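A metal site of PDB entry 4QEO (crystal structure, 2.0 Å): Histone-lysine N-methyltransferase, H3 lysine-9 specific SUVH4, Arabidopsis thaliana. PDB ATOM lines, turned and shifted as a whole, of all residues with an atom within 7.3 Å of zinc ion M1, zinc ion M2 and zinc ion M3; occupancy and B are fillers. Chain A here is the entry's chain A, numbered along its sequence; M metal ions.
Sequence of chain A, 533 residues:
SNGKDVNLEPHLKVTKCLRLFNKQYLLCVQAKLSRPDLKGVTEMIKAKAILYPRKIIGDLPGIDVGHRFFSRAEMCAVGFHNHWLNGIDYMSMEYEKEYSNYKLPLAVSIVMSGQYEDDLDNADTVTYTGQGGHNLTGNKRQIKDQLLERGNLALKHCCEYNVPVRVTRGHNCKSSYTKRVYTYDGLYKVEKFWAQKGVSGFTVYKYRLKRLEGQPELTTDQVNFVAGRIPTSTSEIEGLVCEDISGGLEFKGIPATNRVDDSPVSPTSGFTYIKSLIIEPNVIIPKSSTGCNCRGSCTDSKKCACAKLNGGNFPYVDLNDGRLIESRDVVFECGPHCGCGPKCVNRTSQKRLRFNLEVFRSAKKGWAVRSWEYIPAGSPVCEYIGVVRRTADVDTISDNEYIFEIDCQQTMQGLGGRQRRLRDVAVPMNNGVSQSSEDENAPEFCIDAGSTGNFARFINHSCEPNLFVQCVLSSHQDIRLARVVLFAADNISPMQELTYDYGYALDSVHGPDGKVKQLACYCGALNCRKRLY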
ATOM      1  N   THR A 290      10.563 -15.311  15.028  1.00  0.00           N
ATOM      2  CA  THR A 290      11.068 -15.511  16.383  1.00  0.00           C
ATOM      3  C   THR A 290      10.789 -14.291  17.255  1.00  0.00           C
ATOM      4  O   THR A 290      10.389 -14.421  18.411  1.00  0.00           O
ATOM      5  CB  THR A 290      12.581 -15.793  16.377  1.00  0.00           C
ATOM      6  OG1 THR A 290      12.817 -17.054  15.753  1.00  0.00           O
ATOM      7  CG2 THR A 290      13.115 -15.827  17.807  1.00  0.00           C
ATOM      8  N   GLY A 291      11.018 -13.113  16.710  1.00  0.00           N
ATOM      9  CA  GLY A 291      10.740 -11.888  17.426  1.00  0.00           C
ATOM     10  C   GLY A 291      11.875 -11.434  18.322  1.00  0.00           C
ATOM     11  O   GLY A 291      12.907 -12.095  18.413  1.00  0.00           O
ATOM     12  N   CYS A 292      11.670 -10.289  18.979  1.00  0.00           N
ATOM     13  CA  CYS A 292      12.691  -9.668  19.809  1.00  0.00           C
ATOM     14  C   CYS A 292      12.447  -9.914  21.292  1.00  0.00           C
ATOM     15  O   CYS A 292      11.358 -10.362  21.680  1.00  0.00           O
ATOM     16  CB  CYS A 292      12.718  -8.151  19.524  1.00  0.00           C
ATOM     17  SG  CYS A 292      11.219  -7.235  20.052  1.00  0.00           S
ATOM     18  N   ASN A 293      13.428  -9.602  22.129  1.00  0.00           N
ATOM     19  CA  ASN A 293      13.322  -9.902  23.555  1.00  0.00           C
ATOM     20  C   ASN A 293      13.151  -8.669  24.437  1.00  0.00           C
ATOM     21  O   ASN A 293      13.331  -8.739  25.649  1.00  0.00           O
ATOM     22  CB  ASN A 293      14.512 -10.731  24.046  1.00  0.00           C
ATOM     23  CG  ASN A 293      15.814  -9.953  24.005  1.00  0.00           C
ATOM     24  OD1 ASN A 293      16.052  -9.072  24.827  1.00  0.00           O
ATOM     25  ND2 ASN A 293      16.662 -10.290  23.048  1.00  0.00           N
ATOM     26  N   CYS A 294      12.804  -7.538  23.829  1.00  0.00           N
ATOM     27  CA  CYS A 294      12.654  -6.290  24.578  1.00  0.00           C
ATOM     28  C   CYS A 294      11.480  -6.370  25.555  1.00  0.00           C
ATOM     29  O   CYS A 294      10.534  -7.119  25.332  1.00  0.00           O
ATOM     30  CB  CYS A 294      12.462  -5.121  23.600  1.00  0.00           C
ATOM     31  SG  CYS A 294      13.692  -5.043  22.272  1.00  0.00           S
ATOM     32  N   ARG A 295      11.545  -5.605  26.628  1.00  0.00           N
ATOM     33  CA  ARG A 295      10.438  -5.529  27.568  1.00  0.00           C
ATOM     34  C   ARG A 295       9.695  -4.196  27.428  1.00  0.00           C
ATOM     35  O   ARG A 295      10.315  -3.141  27.312  1.00  0.00           O
ATOM     36  CB  ARG A 295      10.950  -5.658  28.999  1.00  0.00           C
ATOM     37  CG  ARG A 295      11.495  -7.042  29.359  1.00  0.00           C
ATOM     38  CD  ARG A 295      12.390  -6.956  30.580  1.00  0.00           C
ATOM     39  NE  ARG A 295      11.865  -6.017  31.570  1.00  0.00           N
ATOM     40  CZ  ARG A 295      11.562  -6.330  32.826  1.00  0.00           C
ATOM     41  NH1 ARG A 295      11.745  -7.569  33.261  1.00  0.00           N
ATOM     42  NH2 ARG A 295      11.093  -5.407  33.649  1.00  0.00           N
ATOM     43  N   GLY A 296       8.361  -4.252  27.428  1.00  0.00           N
ATOM     44  CA  GLY A 296       7.555  -3.049  27.395  1.00  0.00           C
ATOM     45  C   GLY A 296       7.430  -2.421  26.023  1.00  0.00           C
ATOM     46  O   GLY A 296       6.408  -2.591  25.358  1.00  0.00           O
ATOM     47  N   SER A 297       8.454  -1.687  25.605  1.00  0.00           N
ATOM     48  CA  SER A 297       8.497  -1.095  24.268  1.00  0.00           C
ATOM     49  C   SER A 297       9.892  -1.168  23.671  1.00  0.00           C
ATOM     50  O   SER A 297      10.884  -1.149  24.381  1.00  0.00           O
ATOM     51  CB  SER A 297       8.021   0.356  24.305  1.00  0.00           C
ATOM     52  OG  SER A 297       6.634   0.430  24.576  1.00  0.00           O
ATOM     53  N   CYS A 298       9.970  -1.266  22.346  1.00  0.00           N
ATOM     54  CA  CYS A 298      11.251  -1.390  21.662  1.00  0.00           C
ATOM     55  C   CYS A 298      11.807  -0.015  21.294  1.00  0.00           C
ATOM     56  O   CYS A 298      11.201   0.720  20.502  1.00  0.00           O
ATOM     57  CB  CYS A 298      11.111  -2.258  20.418  1.00  0.00           C
ATOM     58  SG  CYS A 298      10.379  -3.891  20.793  1.00  0.00           S
ATOM     59  N   THR A 299      12.952   0.323  21.896  1.00  0.00           N
ATOM     60  CA  THR A 299      13.523   1.662  21.792  1.00  0.00           C
ATOM     61  C   THR A 299      14.971   1.659  21.302  1.00  0.00           C
ATOM     62  O   THR A 299      15.400   2.555  20.574  1.00  0.00           O
ATOM     63  CB  THR A 299      13.471   2.379  23.152  1.00  0.00           C
ATOM     64  OG1 THR A 299      14.121   1.563  24.146  1.00  0.00           O
ATOM     65  CG2 THR A 299      12.032   2.621  23.565  1.00  0.00           C
ATOM     66  N   ASP A 300      15.725   0.634  21.696  1.00  0.00           N
ATOM     67  CA  ASP A 300      17.125   0.572  21.312  1.00  0.00           C
ATOM     68  C   ASP A 300      17.357  -0.346  20.127  1.00  0.00           C
ATOM     69  O   ASP A 300      17.066  -1.547  20.195  1.00  0.00           O
ATOM     70  CB  ASP A 300      17.984   0.143  22.495  1.00  0.00           C
ATOM     71  CG  ASP A 300      19.358  -0.332  22.093  1.00  0.00           C
ATOM     72  OD1 ASP A 300      19.933   0.192  21.110  1.00  0.00           O
ATOM     73  OD2 ASP A 300      19.890  -1.232  22.780  1.00  0.00           O
ATOM     74  N   LYS A 303      19.790  -3.660  20.883  1.00  0.00           N
ATOM     75  CA  LYS A 303      19.170  -4.858  21.456  1.00  0.00           C
ATOM     76  C   LYS A 303      18.130  -5.502  20.541  1.00  0.00           C
ATOM     77  O   LYS A 303      18.211  -6.705  20.249  1.00  0.00           O
ATOM     78  CB  LYS A 303      18.544  -4.531  22.819  1.00  0.00           C
ATOM     79  CG  LYS A 303      19.573  -4.222  23.905  1.00  0.00           C
ATOM     80  CD  LYS A 303      18.934  -3.560  25.116  1.00  0.00           C
ATOM     81  CE  LYS A 303      19.978  -2.810  25.944  1.00  0.00           C
ATOM     82  NZ  LYS A 303      20.913  -3.703  26.682  1.00  0.00           N
ATOM     83  N   CYS A 304      17.175  -4.704  20.081  1.00  0.00           N
ATOM     84  CA  CYS A 304      16.013  -5.195  19.348  1.00  0.00           C
ATOM     85  C   CYS A 304      16.305  -5.824  17.981  1.00  0.00           C
ATOM     86  O   CYS A 304      16.725  -5.134  17.052  1.00  0.00           O
ATOM     87  CB  CYS A 304      14.986  -4.080  19.154  1.00  0.00           C
ATOM     88  SG  CYS A 304      13.486  -4.714  18.369  1.00  0.00           S
ATOM     89  N   ALA A 305      16.026  -7.115  17.868  1.00  0.00           N
ATOM     90  CA  ALA A 305      16.203  -7.862  16.620  1.00  0.00           C
ATOM     91  C   ALA A 305      15.282  -7.380  15.497  1.00  0.00           C
ATOM     92  O   ALA A 305      15.591  -7.528  14.309  1.00  0.00           O
ATOM     93  CB  ALA A 305      15.961  -9.339  16.867  1.00  0.00           C
ATOM     94  N   CYS A 306      14.127  -6.838  15.849  1.00  0.00           N
ATOM     95  CA  CYS A 306      13.186  -6.426  14.826  1.00  0.00           C
ATOM     96  C   CYS A 306      13.739  -5.185  14.101  1.00  0.00           C
ATOM     97  O   CYS A 306      13.688  -5.073  12.858  1.00  0.00           O
ATOM     98  CB  CYS A 306      11.777  -6.228  15.426  1.00  0.00           C
ATOM     99  SG  CYS A 306      11.131  -7.703  16.394  1.00  0.00           S
ATOM    100  N   ALA A 307      14.350  -4.293  14.874  1.00  0.00           N
ATOM    101  CA  ALA A 307      15.063  -3.153  14.299  1.00  0.00           C
ATOM    102  C   ALA A 307      16.144  -3.642  13.340  1.00  0.00           C
ATOM    103  O   ALA A 307      16.273  -3.125  12.221  1.00  0.00           O
ATOM    104  CB  ALA A 307      15.688  -2.317  15.399  1.00  0.00           C
ATOM    105  N   PHE A 314      14.563   1.776  13.504  1.00  0.00           N
ATOM    106  CA  PHE A 314      13.108   1.715  13.557  1.00  0.00           C
ATOM    107  C   PHE A 314      12.464   2.506  12.415  1.00  0.00           C
ATOM    108  O   PHE A 314      12.823   3.665  12.180  1.00  0.00           O
ATOM    109  CB  PHE A 314      12.587   2.194  14.905  1.00  0.00           C
ATOM    110  CG  PHE A 314      12.996   1.304  16.040  1.00  0.00           C
ATOM    111  CD1 PHE A 314      12.328   0.115  16.278  1.00  0.00           C
ATOM    112  CD2 PHE A 314      14.073   1.645  16.851  1.00  0.00           C
ATOM    113  CE1 PHE A 314      12.723  -0.718  17.319  1.00  0.00           C
ATOM    114  CE2 PHE A 314      14.464   0.821  17.892  1.00  0.00           C
ATOM    115  CZ  PHE A 314      13.780  -0.365  18.129  1.00  0.00           C
ATOM    116  N   PHE A 332       9.301  -4.422   8.986  1.00  0.00           N
ATOM    117  CA  PHE A 332       9.320  -5.558   9.908  1.00  0.00           C
ATOM    118  C   PHE A 332       8.842  -5.126  11.280  1.00  0.00           C
ATOM    119  O   PHE A 332       9.585  -4.515  12.050  1.00  0.00           O
ATOM    120  CB  PHE A 332      10.715  -6.155  10.018  1.00  0.00           C
ATOM    121  CG  PHE A 332      11.181  -6.879   8.787  1.00  0.00           C
ATOM    122  CD1 PHE A 332      10.851  -8.206   8.582  1.00  0.00           C
ATOM    123  CD2 PHE A 332      11.976  -6.240   7.846  1.00  0.00           C
ATOM    124  CE1 PHE A 332      11.291  -8.892   7.455  1.00  0.00           C
ATOM    125  CE2 PHE A 332      12.425  -6.912   6.719  1.00  0.00           C
ATOM    126  CZ  PHE A 332      12.077  -8.235   6.527  1.00  0.00           C
ATOM    127  N   GLU A 333       7.589  -5.450  11.580  1.00  0.00           N
ATOM    128  CA  GLU A 333       7.009  -5.098  12.852  1.00  0.00           C
ATOM    129  C   GLU A 333       7.211  -6.185  13.885  1.00  0.00           C
ATOM    130  O   GLU A 333       7.405  -7.364  13.554  1.00  0.00           O
ATOM    131  CB  GLU A 333       5.509  -4.817  12.696  1.00  0.00           C
ATOM    132  CG  GLU A 333       5.187  -3.423  12.167  1.00  0.00           C
ATOM    133  CD  GLU A 333       3.701  -3.110  12.138  1.00  0.00           C
ATOM    134  OE1 GLU A 333       2.884  -3.987  12.518  1.00  0.00           O
ATOM    135  OE2 GLU A 333       3.347  -1.995  11.735  1.00  0.00           O
ATOM    136  N   CYS A 334       7.159  -5.776  15.147  1.00  0.00           N
ATOM    137  CA  CYS A 334       7.096  -6.710  16.251  1.00  0.00           C
ATOM    138  C   CYS A 334       5.847  -7.582  16.119  1.00  0.00           C
ATOM    139  O   CYS A 334       4.813  -7.145  15.580  1.00  0.00           O
ATOM    140  CB  CYS A 334       7.133  -5.968  17.593  1.00  0.00           C
ATOM    141  SG  CYS A 334       8.734  -5.146  17.966  1.00  0.00           S
ATOM    142  N   GLY A 335       5.952  -8.820  16.579  1.00  0.00           N
ATOM    143  CA  GLY A 335       4.900  -9.796  16.387  1.00  0.00           C
ATOM    144  C   GLY A 335       4.498 -10.551  17.643  1.00  0.00           C
ATOM    145  O   GLY A 335       4.828 -10.130  18.749  1.00  0.00           O
ATOM    146  N   HIS A 337       5.447 -13.259  19.163  1.00  0.00           N
ATOM    147  CA  HIS A 337       6.472 -13.738  20.085  1.00  0.00           C
ATOM    148  C   HIS A 337       7.404 -12.666  20.646  1.00  0.00           C
ATOM    149  O   HIS A 337       8.298 -12.988  21.438  1.00  0.00           O
ATOM    150  CB  HIS A 337       7.290 -14.886  19.451  1.00  0.00           C
ATOM    151  CG  HIS A 337       6.507 -16.140  19.276  1.00  0.00           C
ATOM    152  ND1 HIS A 337       6.128 -16.619  18.042  1.00  0.00           N
ATOM    153  CD2 HIS A 337       5.984 -17.003  20.184  1.00  0.00           C
ATOM    154  CE1 HIS A 337       5.429 -17.728  18.192  1.00  0.00           C
ATOM    155  NE2 HIS A 337       5.328 -17.977  19.483  1.00  0.00           N
ATOM    156  N   CYS A 338       7.236 -11.408  20.247  1.00  0.00           N
ATOM    157  CA  CYS A 338       8.072 -10.344  20.797  1.00  0.00           C
ATOM    158  C   CYS A 338       7.713 -10.076  22.256  1.00  0.00           C
ATOM    159  O   CYS A 338       6.550 -10.197  22.646  1.00  0.00           O
ATOM    160  CB  CYS A 338       7.967  -9.045  19.981  1.00  0.00           C
ATOM    161  SG  CYS A 338       8.613  -9.214  18.304  1.00  0.00           S
ATOM    162  N   GLY A 339       8.712  -9.693  23.048  1.00  0.00           N
ATOM    163  CA  GLY A 339       8.525  -9.485  24.466  1.00  0.00           C
ATOM    164  C   GLY A 339       7.801  -8.191  24.781  1.00  0.00           C
ATOM    165  O   GLY A 339       7.357  -7.993  25.913  1.00  0.00           O
ATOM    166  N   CYS A 340       7.679  -7.318  23.792  1.00  0.00           N
ATOM    167  CA  CYS A 340       7.085  -5.998  23.955  1.00  0.00           C
ATOM    168  C   CYS A 340       5.568  -6.074  23.984  1.00  0.00           C
ATOM    169  O   CYS A 340       4.962  -6.969  23.375  1.00  0.00           O
ATOM    170  CB  CYS A 340       7.522  -5.094  22.802  1.00  0.00           C
ATOM    171  SG  CYS A 340       7.050  -5.747  21.180  1.00  0.00           S
ATOM    172  N   GLY A 341       4.963  -5.127  24.681  1.00  0.00           N
ATOM    173  CA  GLY A 341       3.518  -5.010  24.736  1.00  0.00           C
ATOM    174  C   GLY A 341       2.958  -4.251  23.549  1.00  0.00           C
ATOM    175  O   GLY A 341       3.699  -3.783  22.694  1.00  0.00           O
ATOM    176  N   LYS A 343       1.800  -1.438  23.023  1.00  0.00           N
ATOM    177  CA  LYS A 343       2.089  -0.024  22.857  1.00  0.00           C
ATOM    178  C   LYS A 343       3.370   0.227  22.064  1.00  0.00           C
ATOM    179  O   LYS A 343       3.681   1.361  21.729  1.00  0.00           O
ATOM    180  CB  LYS A 343       2.194   0.661  24.231  1.00  0.00           C
ATOM    181  CG  LYS A 343       0.852   0.912  24.917  1.00  0.00           C
ATOM    182  CD  LYS A 343       1.050   1.655  26.244  1.00  0.00           C
ATOM    183  CE  LYS A 343      -0.260   1.804  27.025  1.00  0.00           C
ATOM    184  NZ  LYS A 343      -0.015   2.300  28.438  1.00  0.00           N
ATOM    185  N   CYS A 344       4.121  -0.838  21.787  1.00  0.00           N
ATOM    186  CA  CYS A 344       5.399  -0.715  21.075  1.00  0.00           C
ATOM    187  C   CYS A 344       5.220   0.057  19.789  1.00  0.00           C
ATOM    188  O   CYS A 344       4.276  -0.182  19.030  1.00  0.00           O
ATOM    189  CB  CYS A 344       6.017  -2.085  20.772  1.00  0.00           C
ATOM    190  SG  CYS A 344       7.565  -1.968  19.830  1.00  0.00           S
ATOM    191  N   VAL A 345       6.124   0.996  19.516  1.00  0.00           N
ATOM    192  CA  VAL A 345       5.978   1.829  18.315  1.00  0.00           C
ATOM    193  C   VAL A 345       6.237   0.997  17.058  1.00  0.00           C
ATOM    194  O   VAL A 345       5.701   1.271  15.975  1.00  0.00           O
ATOM    195  CB  VAL A 345       6.868   3.091  18.395  1.00  0.00           C
ATOM    196  CG1 VAL A 345       6.613   4.020  17.208  1.00  0.00           C
ATOM    197  CG2 VAL A 345       6.586   3.829  19.682  1.00  0.00           C
ATOM    198  N   ASN A 346       7.008  -0.074  17.234  1.00  0.00           N
ATOM    199  CA  ASN A 346       7.223  -0.994  16.133  1.00  0.00           C
ATOM    200  C   ASN A 346       6.055  -1.965  15.915  1.00  0.00           C
ATOM    201  O   ASN A 346       6.169  -2.945  15.186  1.00  0.00           O
ATOM    202  CB  ASN A 346       8.563  -1.733  16.238  1.00  0.00           C
ATOM    203  CG  ASN A 346       9.084  -2.179  14.889  1.00  0.00           C
ATOM    204  OD1 ASN A 346       9.019  -1.444  13.919  1.00  0.00           O
ATOM    205  ND2 ASN A 346       9.563  -3.413  14.818  1.00  0.00           N
ATOM    206  N   ARG A 347       4.924  -1.683  16.558  1.00  0.00           N
ATOM    207  CA  ARG A 347       3.668  -2.306  16.208  1.00  0.00           C
ATOM    208  C   ARG A 347       2.687  -1.275  15.635  1.00  0.00           C
ATOM    209  O   ARG A 347       1.470  -1.486  15.693  1.00  0.00           O
ATOM    210  CB  ARG A 347       3.038  -2.973  17.446  1.00  0.00           C
ATOM    211  CG  ARG A 347       3.916  -4.055  18.102  1.00  0.00           C
ATOM    212  CD  ARG A 347       3.231  -4.592  19.349  1.00  0.00           C
ATOM    213  NE  ARG A 347       3.959  -5.682  20.013  1.00  0.00           N
ATOM    214  CZ  ARG A 347       3.813  -6.968  19.714  1.00  0.00           C
ATOM    215  NH1 ARG A 347       2.998  -7.337  18.730  1.00  0.00           N
ATOM    216  NH2 ARG A 347       4.481  -7.898  20.393  1.00  0.00           N
HETATM  217 ZN    ZN M   1       8.405  -4.193  19.954  1.00  0.00          ZN
HETATM  218 ZN    ZN M   2       9.985  -7.274  18.138  1.00  0.00          ZN
HETATM  219 ZN    ZN M   3      12.325  -5.183  20.305  1.00  0.00          ZN
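Zinc ion M2 is bound by SG of Cys 306 (2.1 Å), SG of Cys 292 (2.3 Å), SG of Cys 338 (2.4 Å) and SG of Cys 334 (2.5 Å). Zinc ion M2 has four donor atoms within binding distance.
The backbone NH (N) of Cys 340 lies within hydrogen-bond range of the backbone carbonyl oxygen (O) of Cys 294, 3.2 Å away. O of Cys 292 is in hydrogen-bond range of N of Gly 339 (3.1 Å). The guanidinium group (NH2) of Arg 347 lies within hydrogen-bond range of the backbone carbonyl oxygen (O) of Cys 340, 3.2 Å away. The side-chain sulfur (SG) of Cys 304 lies close to the backbone NH (N) of Cys 306. The side-chain sulfur of Cys 304 lies close to the backbone NH of Ala 307, at 3.6 Å. The backbone NH of Asn 346 lies close to the side-chain sulfur of Cys 344 (3.3 Å). The backbone carbonyl oxygen (O) of Asn 346 lies within hydrogen-bond range of the backbone NH (N) of Cys 334 (3.0 Å). The backbone NH (N) of Gly 335 sits close to the side-chain sulfur (SG) of Cys 338, at 3.2 Å.
Within 4 Å of zinc ion M2: Cys 292, Cys 306, Cys 334 and Cys 338.
Zinc ion M1 is bound by SG of Cys 298 (2.2 Å), SG of Cys 334 (2.2 Å), SG of Cys 344 (2.4 Å) and SG of Cys 340 (2.4 Å).
Within 4 Å of zinc ion M1: Cys 298, Cys 334, Cys 340 and Cys 344. The nearest printed residue that does not touch zinc ion M1 is Cys 292 (4.1 Å).
Within 4 Å of zinc ion M3: Cys 292, Cys 294, Cys 298 and Cys 304. Along chain A the residues within 4 Å of zinc ion M3 span positions 292 to 304.
Zinc ion M3 is bound by the side-chain sulfur (SG) of Cys 304 (2.3 Å). Zinc ion M3 is bound by SG of Cys 292 (2.3 Å). Zinc ion M3 is bound by SG of Cys 298, 2.4 Å away. The side-chain sulfur (SG) of Cys 294 is bound to zinc ion M3 (2.4 Å).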
